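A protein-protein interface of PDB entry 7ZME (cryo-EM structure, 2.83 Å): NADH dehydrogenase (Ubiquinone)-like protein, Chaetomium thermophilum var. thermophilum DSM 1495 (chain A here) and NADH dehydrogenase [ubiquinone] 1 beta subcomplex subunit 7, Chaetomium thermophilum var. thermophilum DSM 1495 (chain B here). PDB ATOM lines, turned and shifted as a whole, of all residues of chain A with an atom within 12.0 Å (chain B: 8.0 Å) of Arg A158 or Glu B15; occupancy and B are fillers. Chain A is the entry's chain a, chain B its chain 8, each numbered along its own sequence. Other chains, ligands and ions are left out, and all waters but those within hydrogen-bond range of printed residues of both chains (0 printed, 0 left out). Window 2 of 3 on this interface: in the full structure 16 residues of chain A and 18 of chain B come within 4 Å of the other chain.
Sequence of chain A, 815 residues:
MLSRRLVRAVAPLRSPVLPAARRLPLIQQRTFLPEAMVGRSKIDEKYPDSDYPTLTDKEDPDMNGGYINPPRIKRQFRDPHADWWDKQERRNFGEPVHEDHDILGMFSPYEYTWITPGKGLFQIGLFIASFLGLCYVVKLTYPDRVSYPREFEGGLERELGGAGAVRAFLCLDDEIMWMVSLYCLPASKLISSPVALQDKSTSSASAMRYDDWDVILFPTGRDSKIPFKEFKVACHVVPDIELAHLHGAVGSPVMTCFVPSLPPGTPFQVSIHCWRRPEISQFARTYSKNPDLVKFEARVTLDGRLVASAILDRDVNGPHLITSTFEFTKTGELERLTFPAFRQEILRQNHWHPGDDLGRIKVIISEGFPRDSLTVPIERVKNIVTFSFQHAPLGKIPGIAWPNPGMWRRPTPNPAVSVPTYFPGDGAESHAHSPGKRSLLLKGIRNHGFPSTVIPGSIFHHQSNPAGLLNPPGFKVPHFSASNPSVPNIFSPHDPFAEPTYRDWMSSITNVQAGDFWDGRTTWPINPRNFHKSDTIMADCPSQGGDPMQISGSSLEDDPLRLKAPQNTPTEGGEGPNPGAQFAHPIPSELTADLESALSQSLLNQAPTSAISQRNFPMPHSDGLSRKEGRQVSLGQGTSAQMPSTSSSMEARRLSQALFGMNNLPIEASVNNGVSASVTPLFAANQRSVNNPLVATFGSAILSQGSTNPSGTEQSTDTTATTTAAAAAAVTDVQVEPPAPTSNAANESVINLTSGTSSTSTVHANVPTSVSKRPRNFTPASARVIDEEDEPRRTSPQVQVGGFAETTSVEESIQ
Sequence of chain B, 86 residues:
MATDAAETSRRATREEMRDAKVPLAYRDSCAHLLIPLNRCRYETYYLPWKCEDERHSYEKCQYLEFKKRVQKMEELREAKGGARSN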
ATOM      1  N   PHE A 152      -0.185  21.928   7.097  1.00  0.00           N
ATOM      2  CA  PHE A 152      -0.252  20.533   7.509  1.00  0.00           C
ATOM      3  C   PHE A 152       0.745  19.732   6.686  1.00  0.00           C
ATOM      4  O   PHE A 152       0.718  19.784   5.452  1.00  0.00           O
ATOM      5  CB  PHE A 152      -1.667  19.985   7.339  1.00  0.00           C
ATOM      6  CG  PHE A 152      -2.646  20.526   8.339  1.00  0.00           C
ATOM      7  CD1 PHE A 152      -2.581  20.140   9.667  1.00  0.00           C
ATOM      8  CD2 PHE A 152      -3.627  21.421   7.953  1.00  0.00           C
ATOM      9  CE1 PHE A 152      -3.476  20.631  10.587  1.00  0.00           C
ATOM     10  CE2 PHE A 152      -4.525  21.917   8.869  1.00  0.00           C
ATOM     11  CZ  PHE A 152      -4.450  21.522  10.190  1.00  0.00           C
ATOM     12  N   GLU A 153       1.620  18.997   7.369  1.00  0.00           N
ATOM     13  CA  GLU A 153       2.648  18.217   6.690  1.00  0.00           C
ATOM     14  C   GLU A 153       1.996  17.116   5.864  1.00  0.00           C
ATOM     15  O   GLU A 153       1.358  16.213   6.414  1.00  0.00           O
ATOM     16  CB  GLU A 153       3.620  17.624   7.705  1.00  0.00           C
ATOM     17  CG  GLU A 153       4.865  17.004   7.088  1.00  0.00           C
ATOM     18  CD  GLU A 153       4.667  15.551   6.703  1.00  0.00           C
ATOM     19  OE1 GLU A 153       3.829  14.875   7.336  1.00  0.00           O
ATOM     20  OE2 GLU A 153       5.349  15.085   5.765  1.00  0.00           O
ATOM     21  N   GLY A 154       2.156  17.191   4.545  1.00  0.00           N
ATOM     22  CA  GLY A 154       1.544  16.236   3.650  1.00  0.00           C
ATOM     23  C   GLY A 154       0.069  16.452   3.407  1.00  0.00           C
ATOM     24  O   GLY A 154      -0.550  15.643   2.701  1.00  0.00           O
ATOM     25  N   GLY A 155      -0.515  17.510   3.963  1.00  0.00           N
ATOM     26  CA  GLY A 155      -1.922  17.786   3.761  1.00  0.00           C
ATOM     27  C   GLY A 155      -2.861  16.785   4.385  1.00  0.00           C
ATOM     28  O   GLY A 155      -4.023  16.716   3.984  1.00  0.00           O
ATOM     29  N   LEU A 156      -2.390  16.010   5.362  1.00  0.00           N
ATOM     30  CA  LEU A 156      -3.196  14.962   5.993  1.00  0.00           C
ATOM     31  C   LEU A 156      -3.751  14.008   4.942  1.00  0.00           C
ATOM     32  O   LEU A 156      -4.911  13.603   4.991  1.00  0.00           O
ATOM     33  CB  LEU A 156      -4.320  15.570   6.835  1.00  0.00           C
ATOM     34  CG  LEU A 156      -4.087  15.986   8.289  1.00  0.00           C
ATOM     35  CD1 LEU A 156      -3.836  14.788   9.158  1.00  0.00           C
ATOM     36  CD2 LEU A 156      -2.921  16.933   8.395  1.00  0.00           C
ATOM     37  N   GLU A 157      -2.904  13.651   3.977  1.00  0.00           N
ATOM     38  CA  GLU A 157      -3.365  12.931   2.793  1.00  0.00           C
ATOM     39  C   GLU A 157      -3.949  11.570   3.157  1.00  0.00           C
ATOM     40  O   GLU A 157      -5.135  11.307   2.927  1.00  0.00           O
ATOM     41  CB  GLU A 157      -2.209  12.776   1.803  1.00  0.00           C
ATOM     42  CG  GLU A 157      -2.579  12.077   0.507  1.00  0.00           C
ATOM     43  CD  GLU A 157      -3.570  12.869  -0.322  1.00  0.00           C
ATOM     44  OE1 GLU A 157      -3.611  14.109  -0.185  1.00  0.00           O
ATOM     45  OE2 GLU A 157      -4.307  12.249  -1.117  1.00  0.00           O
ATOM     46  N   ARG A 158      -3.126  10.690   3.729  1.00  0.00           N
ATOM     47  CA  ARG A 158      -3.561   9.318   3.971  1.00  0.00           C
ATOM     48  C   ARG A 158      -4.661   9.256   5.023  1.00  0.00           C
ATOM     49  O   ARG A 158      -5.689   8.599   4.820  1.00  0.00           O
ATOM     50  CB  ARG A 158      -2.367   8.462   4.392  1.00  0.00           C
ATOM     51  CG  ARG A 158      -1.206   8.490   3.414  1.00  0.00           C
ATOM     52  CD  ARG A 158      -0.199   7.393   3.723  1.00  0.00           C
ATOM     53  NE  ARG A 158       0.680   7.754   4.831  1.00  0.00           N
ATOM     54  CZ  ARG A 158       0.648   7.177   6.027  1.00  0.00           C
ATOM     55  NH1 ARG A 158       1.487   7.568   6.976  1.00  0.00           N
ATOM     56  NH2 ARG A 158      -0.222   6.209   6.275  1.00  0.00           N
ATOM     57  N   GLU A 159      -4.470   9.943   6.144  1.00  0.00           N
ATOM     58  CA  GLU A 159      -5.324   9.772   7.312  1.00  0.00           C
ATOM     59  C   GLU A 159      -6.584  10.627   7.284  1.00  0.00           C
ATOM     60  O   GLU A 159      -7.373  10.562   8.232  1.00  0.00           O
ATOM     61  CB  GLU A 159      -4.525  10.040   8.593  1.00  0.00           C
ATOM     62  CG  GLU A 159      -3.859  11.396   8.678  1.00  0.00           C
ATOM     63  CD  GLU A 159      -2.586  11.490   7.850  1.00  0.00           C
ATOM     64  OE1 GLU A 159      -1.933  12.554   7.877  1.00  0.00           O
ATOM     65  OE2 GLU A 159      -2.233  10.499   7.177  1.00  0.00           O
ATOM     66  N   LEU A 160      -6.807  11.410   6.230  1.00  0.00           N
ATOM     67  CA  LEU A 160      -8.101  12.035   6.000  1.00  0.00           C
ATOM     68  C   LEU A 160      -8.911  11.308   4.938  1.00  0.00           C
ATOM     69  O   LEU A 160      -9.904  11.851   4.445  1.00  0.00           O
ATOM     70  CB  LEU A 160      -7.937  13.506   5.620  1.00  0.00           C
ATOM     71  CG  LEU A 160      -7.785  14.475   6.789  1.00  0.00           C
ATOM     72  CD1 LEU A 160      -7.768  15.898   6.287  1.00  0.00           C
ATOM     73  CD2 LEU A 160      -8.915  14.270   7.768  1.00  0.00           C
ATOM     74  N   GLY A 161      -8.511  10.095   4.578  1.00  0.00           N
ATOM     75  CA  GLY A 161      -9.244   9.296   3.624  1.00  0.00           C
ATOM     76  C   GLY A 161      -8.574   9.081   2.288  1.00  0.00           C
ATOM     77  O   GLY A 161      -9.204   8.522   1.386  1.00  0.00           O
ATOM     78  N   GLY A 162      -7.325   9.500   2.126  1.00  0.00           N
ATOM     79  CA  GLY A 162      -6.647   9.339   0.861  1.00  0.00           C
ATOM     80  C   GLY A 162      -7.066  10.388  -0.150  1.00  0.00           C
ATOM     81  O   GLY A 162      -7.755  11.364   0.155  1.00  0.00           O
ATOM     82  N   ALA A 163      -6.627  10.167  -1.392  1.00  0.00           N
ATOM     83  CA  ALA A 163      -6.955  11.086  -2.476  1.00  0.00           C
ATOM     84  C   ALA A 163      -8.443  11.100  -2.795  1.00  0.00           C
ATOM     85  O   ALA A 163      -8.918  12.052  -3.423  1.00  0.00           O
ATOM     86  CB  ALA A 163      -6.158  10.726  -3.729  1.00  0.00           C
ATOM     87  N   GLY A 164      -9.182  10.077  -2.376  1.00  0.00           N
ATOM     88  CA  GLY A 164     -10.608  10.014  -2.605  1.00  0.00           C
ATOM     89  C   GLY A 164     -11.450  10.858  -1.680  1.00  0.00           C
ATOM     90  O   GLY A 164     -12.664  10.956  -1.875  1.00  0.00           O
ATOM     91  N   ALA A 165     -10.841  11.477  -0.675  1.00  0.00           N
ATOM     92  CA  ALA A 165     -11.542  12.348   0.253  1.00  0.00           C
ATOM     93  C   ALA A 165     -10.857  13.707   0.275  1.00  0.00           C
ATOM     94  O   ALA A 165      -9.810  13.910  -0.345  1.00  0.00           O
ATOM     95  CB  ALA A 165     -11.591  11.740   1.661  1.00  0.00           C
ATOM     96  N   VAL A 166     -11.465  14.648   0.997  1.00  0.00           N
ATOM     97  CA  VAL A 166     -10.903  15.988   1.097  1.00  0.00           C
ATOM     98  C   VAL A 166      -9.671  15.962   1.991  1.00  0.00           C
ATOM     99  O   VAL A 166      -9.609  15.219   2.981  1.00  0.00           O
ATOM    100  CB  VAL A 166     -11.963  16.979   1.614  1.00  0.00           C
ATOM    101  CG1 VAL A 166     -12.357  16.655   3.047  1.00  0.00           C
ATOM    102  CG2 VAL A 166     -11.460  18.411   1.500  1.00  0.00           C
ATOM    103  N   ARG A 167      -8.672  16.760   1.632  1.00  0.00           N
ATOM    104  CA  ARG A 167      -7.414  16.847   2.359  1.00  0.00           C
ATOM    105  C   ARG A 167      -7.359  18.154   3.141  1.00  0.00           C
ATOM    106  O   ARG A 167      -8.280  18.974   3.097  1.00  0.00           O
ATOM    107  CB  ARG A 167      -6.230  16.732   1.397  1.00  0.00           C
ATOM    108  CG  ARG A 167      -6.227  17.780   0.297  1.00  0.00           C
ATOM    109  CD  ARG A 167      -5.414  17.325  -0.901  1.00  0.00           C
ATOM    110  NE  ARG A 167      -4.029  17.781  -0.828  1.00  0.00           N
ATOM    111  CZ  ARG A 167      -3.597  18.940  -1.314  1.00  0.00           C
ATOM    112  NH1 ARG A 167      -4.445  19.766  -1.911  1.00  0.00           N
ATOM    113  NH2 ARG A 167      -2.319  19.273  -1.203  1.00  0.00           N
ATOM    114  N   ALA A 168      -6.260  18.342   3.858  1.00  0.00           N
ATOM    115  CA  ALA A 168      -6.041  19.523   4.673  1.00  0.00           C
ATOM    116  C   ALA A 168      -5.213  20.547   3.896  1.00  0.00           C
ATOM    117  O   ALA A 168      -4.954  20.396   2.698  1.00  0.00           O
ATOM    118  CB  ALA A 168      -5.383  19.122   5.993  1.00  0.00           C
ATOM    119  N   PHE A 169      -4.789  21.606   4.583  1.00  0.00           N
ATOM    120  CA  PHE A 169      -4.070  22.702   3.948  1.00  0.00           C
ATOM    121  C   PHE A 169      -2.597  22.349   3.789  1.00  0.00           C
ATOM    122  O   PHE A 169      -1.931  21.986   4.762  1.00  0.00           O
ATOM    123  CB  PHE A 169      -4.226  23.975   4.782  1.00  0.00           C
ATOM    124  CG  PHE A 169      -4.112  25.246   3.991  1.00  0.00           C
ATOM    125  CD1 PHE A 169      -5.165  25.685   3.205  1.00  0.00           C
ATOM    126  CD2 PHE A 169      -2.956  26.004   4.040  1.00  0.00           C
ATOM    127  CE1 PHE A 169      -5.064  26.857   2.480  1.00  0.00           C
ATOM    128  CE2 PHE A 169      -2.849  27.176   3.316  1.00  0.00           C
ATOM    129  CZ  PHE A 169      -3.904  27.603   2.535  1.00  0.00           C
ATOM    130  N   LEU A 170      -2.085  22.456   2.560  1.00  0.00           N
ATOM    131  CA  LEU A 170      -0.682  22.131   2.292  1.00  0.00           C
ATOM    132  C   LEU A 170      -0.229  22.897   1.050  1.00  0.00           C
ATOM    133  O   LEU A 170      -0.555  22.503  -0.075  1.00  0.00           O
ATOM    134  CB  LEU A 170      -0.493  20.631   2.116  1.00  0.00           C
ATOM    135  CG  LEU A 170       0.823  20.178   1.478  1.00  0.00           C
ATOM    136  CD1 LEU A 170       1.980  20.319   2.457  1.00  0.00           C
ATOM    137  CD2 LEU A 170       0.717  18.753   0.955  1.00  0.00           C
ATOM    138  N   ALA B  12       7.255  14.761  15.672  1.00  0.00           N
ATOM    139  CA  ALA B  12       6.709  13.417  15.828  1.00  0.00           C
ATOM    140  C   ALA B  12       6.219  12.923  14.471  1.00  0.00           C
ATOM    141  O   ALA B  12       5.285  13.491  13.897  1.00  0.00           O
ATOM    142  CB  ALA B  12       5.581  13.406  16.856  1.00  0.00           C
ATOM    143  N   THR B  13       6.847  11.866  13.966  1.00  0.00           N
ATOM    144  CA  THR B  13       6.443  11.288  12.695  1.00  0.00           C
ATOM    145  C   THR B  13       5.090  10.596  12.829  1.00  0.00           C
ATOM    146  O   THR B  13       4.672  10.193  13.917  1.00  0.00           O
ATOM    147  CB  THR B  13       7.488  10.293  12.194  1.00  0.00           C
ATOM    148  OG1 THR B  13       7.620   9.221  13.135  1.00  0.00           O
ATOM    149  CG2 THR B  13       8.835  10.980  12.024  1.00  0.00           C
ATOM    150  N   ARG B  14       4.411  10.449  11.687  1.00  0.00           N
ATOM    151  CA  ARG B  14       3.048   9.923  11.675  1.00  0.00           C
ATOM    152  C   ARG B  14       2.965   8.522  12.261  1.00  0.00           C
ATOM    153  O   ARG B  14       1.931   8.151  12.830  1.00  0.00           O
ATOM    154  CB  ARG B  14       2.507   9.914  10.247  1.00  0.00           C
ATOM    155  CG  ARG B  14       2.323  11.286   9.625  1.00  0.00           C
ATOM    156  CD  ARG B  14       1.806  11.150   8.203  1.00  0.00           C
ATOM    157  NE  ARG B  14       1.614  12.443   7.553  1.00  0.00           N
ATOM    158  CZ  ARG B  14       1.224  12.588   6.292  1.00  0.00           C
ATOM    159  NH1 ARG B  14       1.074  13.800   5.780  1.00  0.00           N
ATOM    160  NH2 ARG B  14       0.983  11.522   5.543  1.00  0.00           N
ATOM    161  N   GLU B  15       4.029   7.727  12.127  1.00  0.00           N
ATOM    162  CA  GLU B  15       3.973   6.326  12.533  1.00  0.00           C
ATOM    163  C   GLU B  15       3.695   6.187  14.026  1.00  0.00           C
ATOM    164  O   GLU B  15       2.855   5.381  14.441  1.00  0.00           O
ATOM    165  CB  GLU B  15       5.275   5.621  12.154  1.00  0.00           C
ATOM    166  CG  GLU B  15       5.273   5.035  10.751  1.00  0.00           C
ATOM    167  CD  GLU B  15       5.027   6.080   9.677  1.00  0.00           C
ATOM    168  OE1 GLU B  15       5.503   7.224   9.836  1.00  0.00           O
ATOM    169  OE2 GLU B  15       4.357   5.756   8.675  1.00  0.00           O
ATOM    170  N   GLU B  16       4.344   7.027  14.842  1.00  0.00           N
ATOM    171  CA  GLU B  16       4.074   7.012  16.308  1.00  0.00           C
ATOM    172  C   GLU B  16       2.984   8.038  16.617  1.00  0.00           C
ATOM    173  O   GLU B  16       2.637   8.193  17.803  1.00  0.00           O
ATOM    174  CB  GLU B  16       5.345   7.325  17.099  1.00  0.00           C
ATOM    175  CG  GLU B  16       5.824   8.757  16.943  1.00  0.00           C
ATOM    176  CD  GLU B  16       7.140   8.901  16.200  1.00  0.00           C
ATOM    177  OE1 GLU B  16       7.665  10.030  16.145  1.00  0.00           O
ATOM    178  OE2 GLU B  16       7.633   7.886  15.673  1.00  0.00           O
ATOM    179  N   MET B  17       2.453   8.696  15.587  1.00  0.00           N
ATOM    180  CA  MET B  17       1.450   9.731  15.775  1.00  0.00           C
ATOM    181  C   MET B  17       0.067   9.295  15.311  1.00  0.00           C
ATOM    182  O   MET B  17      -0.934   9.847  15.783  1.00  0.00           O
ATOM    183  CB  MET B  17       1.898  10.991  15.033  1.00  0.00           C
ATOM    184  CG  MET B  17       1.044  12.211  15.165  1.00  0.00           C
ATOM    185  SD  MET B  17       1.914  13.501  14.263  1.00  0.00           S
ATOM    186  CE  MET B  17       0.771  14.846  14.402  1.00  0.00           C
ATOM    187  N   ARG B  18      -0.005   8.321  14.404  1.00  0.00           N
ATOM    188  CA  ARG B  18      -1.255   7.602  14.190  1.00  0.00           C
ATOM    189  C   ARG B  18      -1.528   6.646  15.343  1.00  0.00           C
ATOM    190  O   ARG B  18      -2.679   6.472  15.756  1.00  0.00           O
ATOM    191  CB  ARG B  18      -1.201   6.848  12.861  1.00  0.00           C
ATOM    192  CG  ARG B  18      -2.358   5.887  12.633  1.00  0.00           C
ATOM    193  CD  ARG B  18      -1.926   4.435  12.804  1.00  0.00           C
ATOM    194  NE  ARG B  18      -0.647   4.156  12.160  1.00  0.00           N
ATOM    195  CZ  ARG B  18      -0.506   3.867  10.871  1.00  0.00           C
ATOM    196  NH1 ARG B  18       0.697   3.625  10.371  1.00  0.00           N
ATOM    197  NH2 ARG B  18      -1.570   3.816  10.081  1.00  0.00           N
ATOM    198  N   ASP B  19      -0.474   6.023  15.876  1.00  0.00           N
ATOM    199  CA  ASP B  19      -0.631   5.126  17.017  1.00  0.00           C
ATOM    200  C   ASP B  19      -1.056   5.882  18.269  1.00  0.00           C
ATOM    201  O   ASP B  19      -1.749   5.320  19.124  1.00  0.00           O
ATOM    202  CB  ASP B  19       0.673   4.374  17.272  1.00  0.00           C
ATOM    203  CG  ASP B  19       0.945   3.310  16.227  1.00  0.00           C
ATOM    204  OD1 ASP B  19       0.349   3.383  15.131  1.00  0.00           O
ATOM    205  OD2 ASP B  19       1.759   2.401  16.496  1.00  0.00           O
ATOM    206  N   ALA B  20      -0.652   7.147  18.398  1.00  0.00           N
ATOM    207  CA  ALA B  20      -1.042   7.944  19.554  1.00  0.00           C
ATOM    208  C   ALA B  20      -2.509   8.345  19.513  1.00  0.00           C
ATOM    209  O   ALA B  20      -3.048   8.770  20.540  1.00  0.00           O
ATOM    210  CB  ALA B  20      -0.166   9.191  19.653  1.00  0.00           C
ATOM    211  N   LYS B  21      -3.159   8.221  18.353  1.00  0.00           N
ATOM    212  CA  LYS B  21      -4.582   8.527  18.193  1.00  0.00           C
ATOM    213  C   LYS B  21      -4.898   9.967  18.592  1.00  0.00           C
ATOM    214  O   LYS B  21      -5.827  10.233  19.354  1.00  0.00           O
ATOM    215  CB  LYS B  21      -5.448   7.542  18.985  1.00  0.00           C
ATOM    216  CG  LYS B  21      -5.390   6.110  18.486  1.00  0.00           C
ATOM    217  CD  LYS B  21      -6.287   5.207  19.317  1.00  0.00           C
ATOM    218  CE  LYS B  21      -6.307   3.790  18.771  1.00  0.00           C
ATOM    219  NZ  LYS B  21      -4.985   3.120  18.912  1.00  0.00           N
ATOM    220  N   LEU B  24      -7.438  14.644  14.174  1.00  0.00           N
ATOM    221  CA  LEU B  24      -6.952  15.016  12.848  1.00  0.00           C
ATOM    222  C   LEU B  24      -6.565  16.487  12.791  1.00  0.00           C
ATOM    223  O   LEU B  24      -5.514  16.844  12.248  1.00  0.00           O
ATOM    224  CB  LEU B  24      -8.007  14.732  11.780  1.00  0.00           C
ATOM    225  CG  LEU B  24      -8.177  13.338  11.178  1.00  0.00           C
ATOM    226  CD1 LEU B  24      -6.921  12.912  10.424  1.00  0.00           C
ATOM    227  CD2 LEU B  24      -8.598  12.320  12.195  1.00  0.00           C
ATOM    228  N   ARG B  27      -3.055  17.292  13.956  1.00  0.00           N
ATOM    229  CA  ARG B  27      -1.939  16.565  13.359  1.00  0.00           C
ATOM    230  C   ARG B  27      -0.982  17.569  12.724  1.00  0.00           C
ATOM    231  O   ARG B  27      -0.967  17.790  11.511  1.00  0.00           O
ATOM    232  CB  ARG B  27      -2.432  15.554  12.333  1.00  0.00           C
ATOM    233  CG  ARG B  27      -3.352  14.474  12.866  1.00  0.00           C
ATOM    234  CD  ARG B  27      -2.600  13.190  13.127  1.00  0.00           C
ATOM    235  NE  ARG B  27      -3.357  12.289  13.985  1.00  0.00           N
ATOM    236  CZ  ARG B  27      -4.003  11.213  13.555  1.00  0.00           C
ATOM    237  NH1 ARG B  27      -3.981  10.891  12.269  1.00  0.00           N
ATOM    238  NH2 ARG B  27      -4.667  10.454  14.415  1.00  0.00           N
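OE1 of Glu A159 lies within salt-bridge range of NE of Arg B14, 3.6 Å away. The guanidinium group (NH1) of Arg A158 lies within salt-bridge range of the side-chain carboxylate (OE2) of Glu B15, 3.8 Å away. The guanidinium group (NE) of Arg B14 lies within salt-bridge range of the side-chain carboxylate (OE1) of Glu A153.
The backbone carbonyl oxygen (O) of Phe A169 lies within hydrogen-bond range of the backbone NH (N) of Phe A152 (2.9 Å).
CD1 of Phe A152 touches O of Arg B27, at 3.4 Å. Gly A154 touches Arg B14. Leu A156 touches Leu B24 (CD1 to CD1, 3.8 Å). Arg B27 touches Leu A156. Arg A158 touches Arg B14. CD1 of Leu B24 touches O of Glu A159 (3.2 Å). Glu A159 touches Arg B27 (CG to NH1, 3.6 Å). Leu A160 touches Leu B24 (CD2 to CD1, 3.6 Å).
Of the printed residues of chain B, Glu A153 touches Arg B14 (2.5 Å). Of chain B, only Arg B14 (3.8 Å) and Glu B15 (3.8 Å) come within 4 Å of Arg A158. Of the printed residues of chain B, Glu A159 touches Arg B14, Leu B24 and Arg B27. Ala B12 touches none of the printed residues of chain A. Printed residues of chain A within 4 Å of Glu B15: Arg A158. No residue of chain A comes within 4 Å of Glu B16. No residue of chain A comes within 4 Å of Arg B18. The nearest printed residue of chain B that does not touch Leu A156 is Arg B14 (4.1 Å).
Hydrophobic or aromatic side chains of chain A that line the printed part of chain B: Phe A152, Leu A156 and Leu A160. Of the 12 printed residues of chain B, 4 touch a printed residue of chain A. Among the printed residues, Asp or Glu carboxylates within 4 Å of a Lys or Arg side-chain nitrogen of the other chain: Glu A153 with Arg B14, Arg A158 with Glu B15 and Glu A159 with Arg B14.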
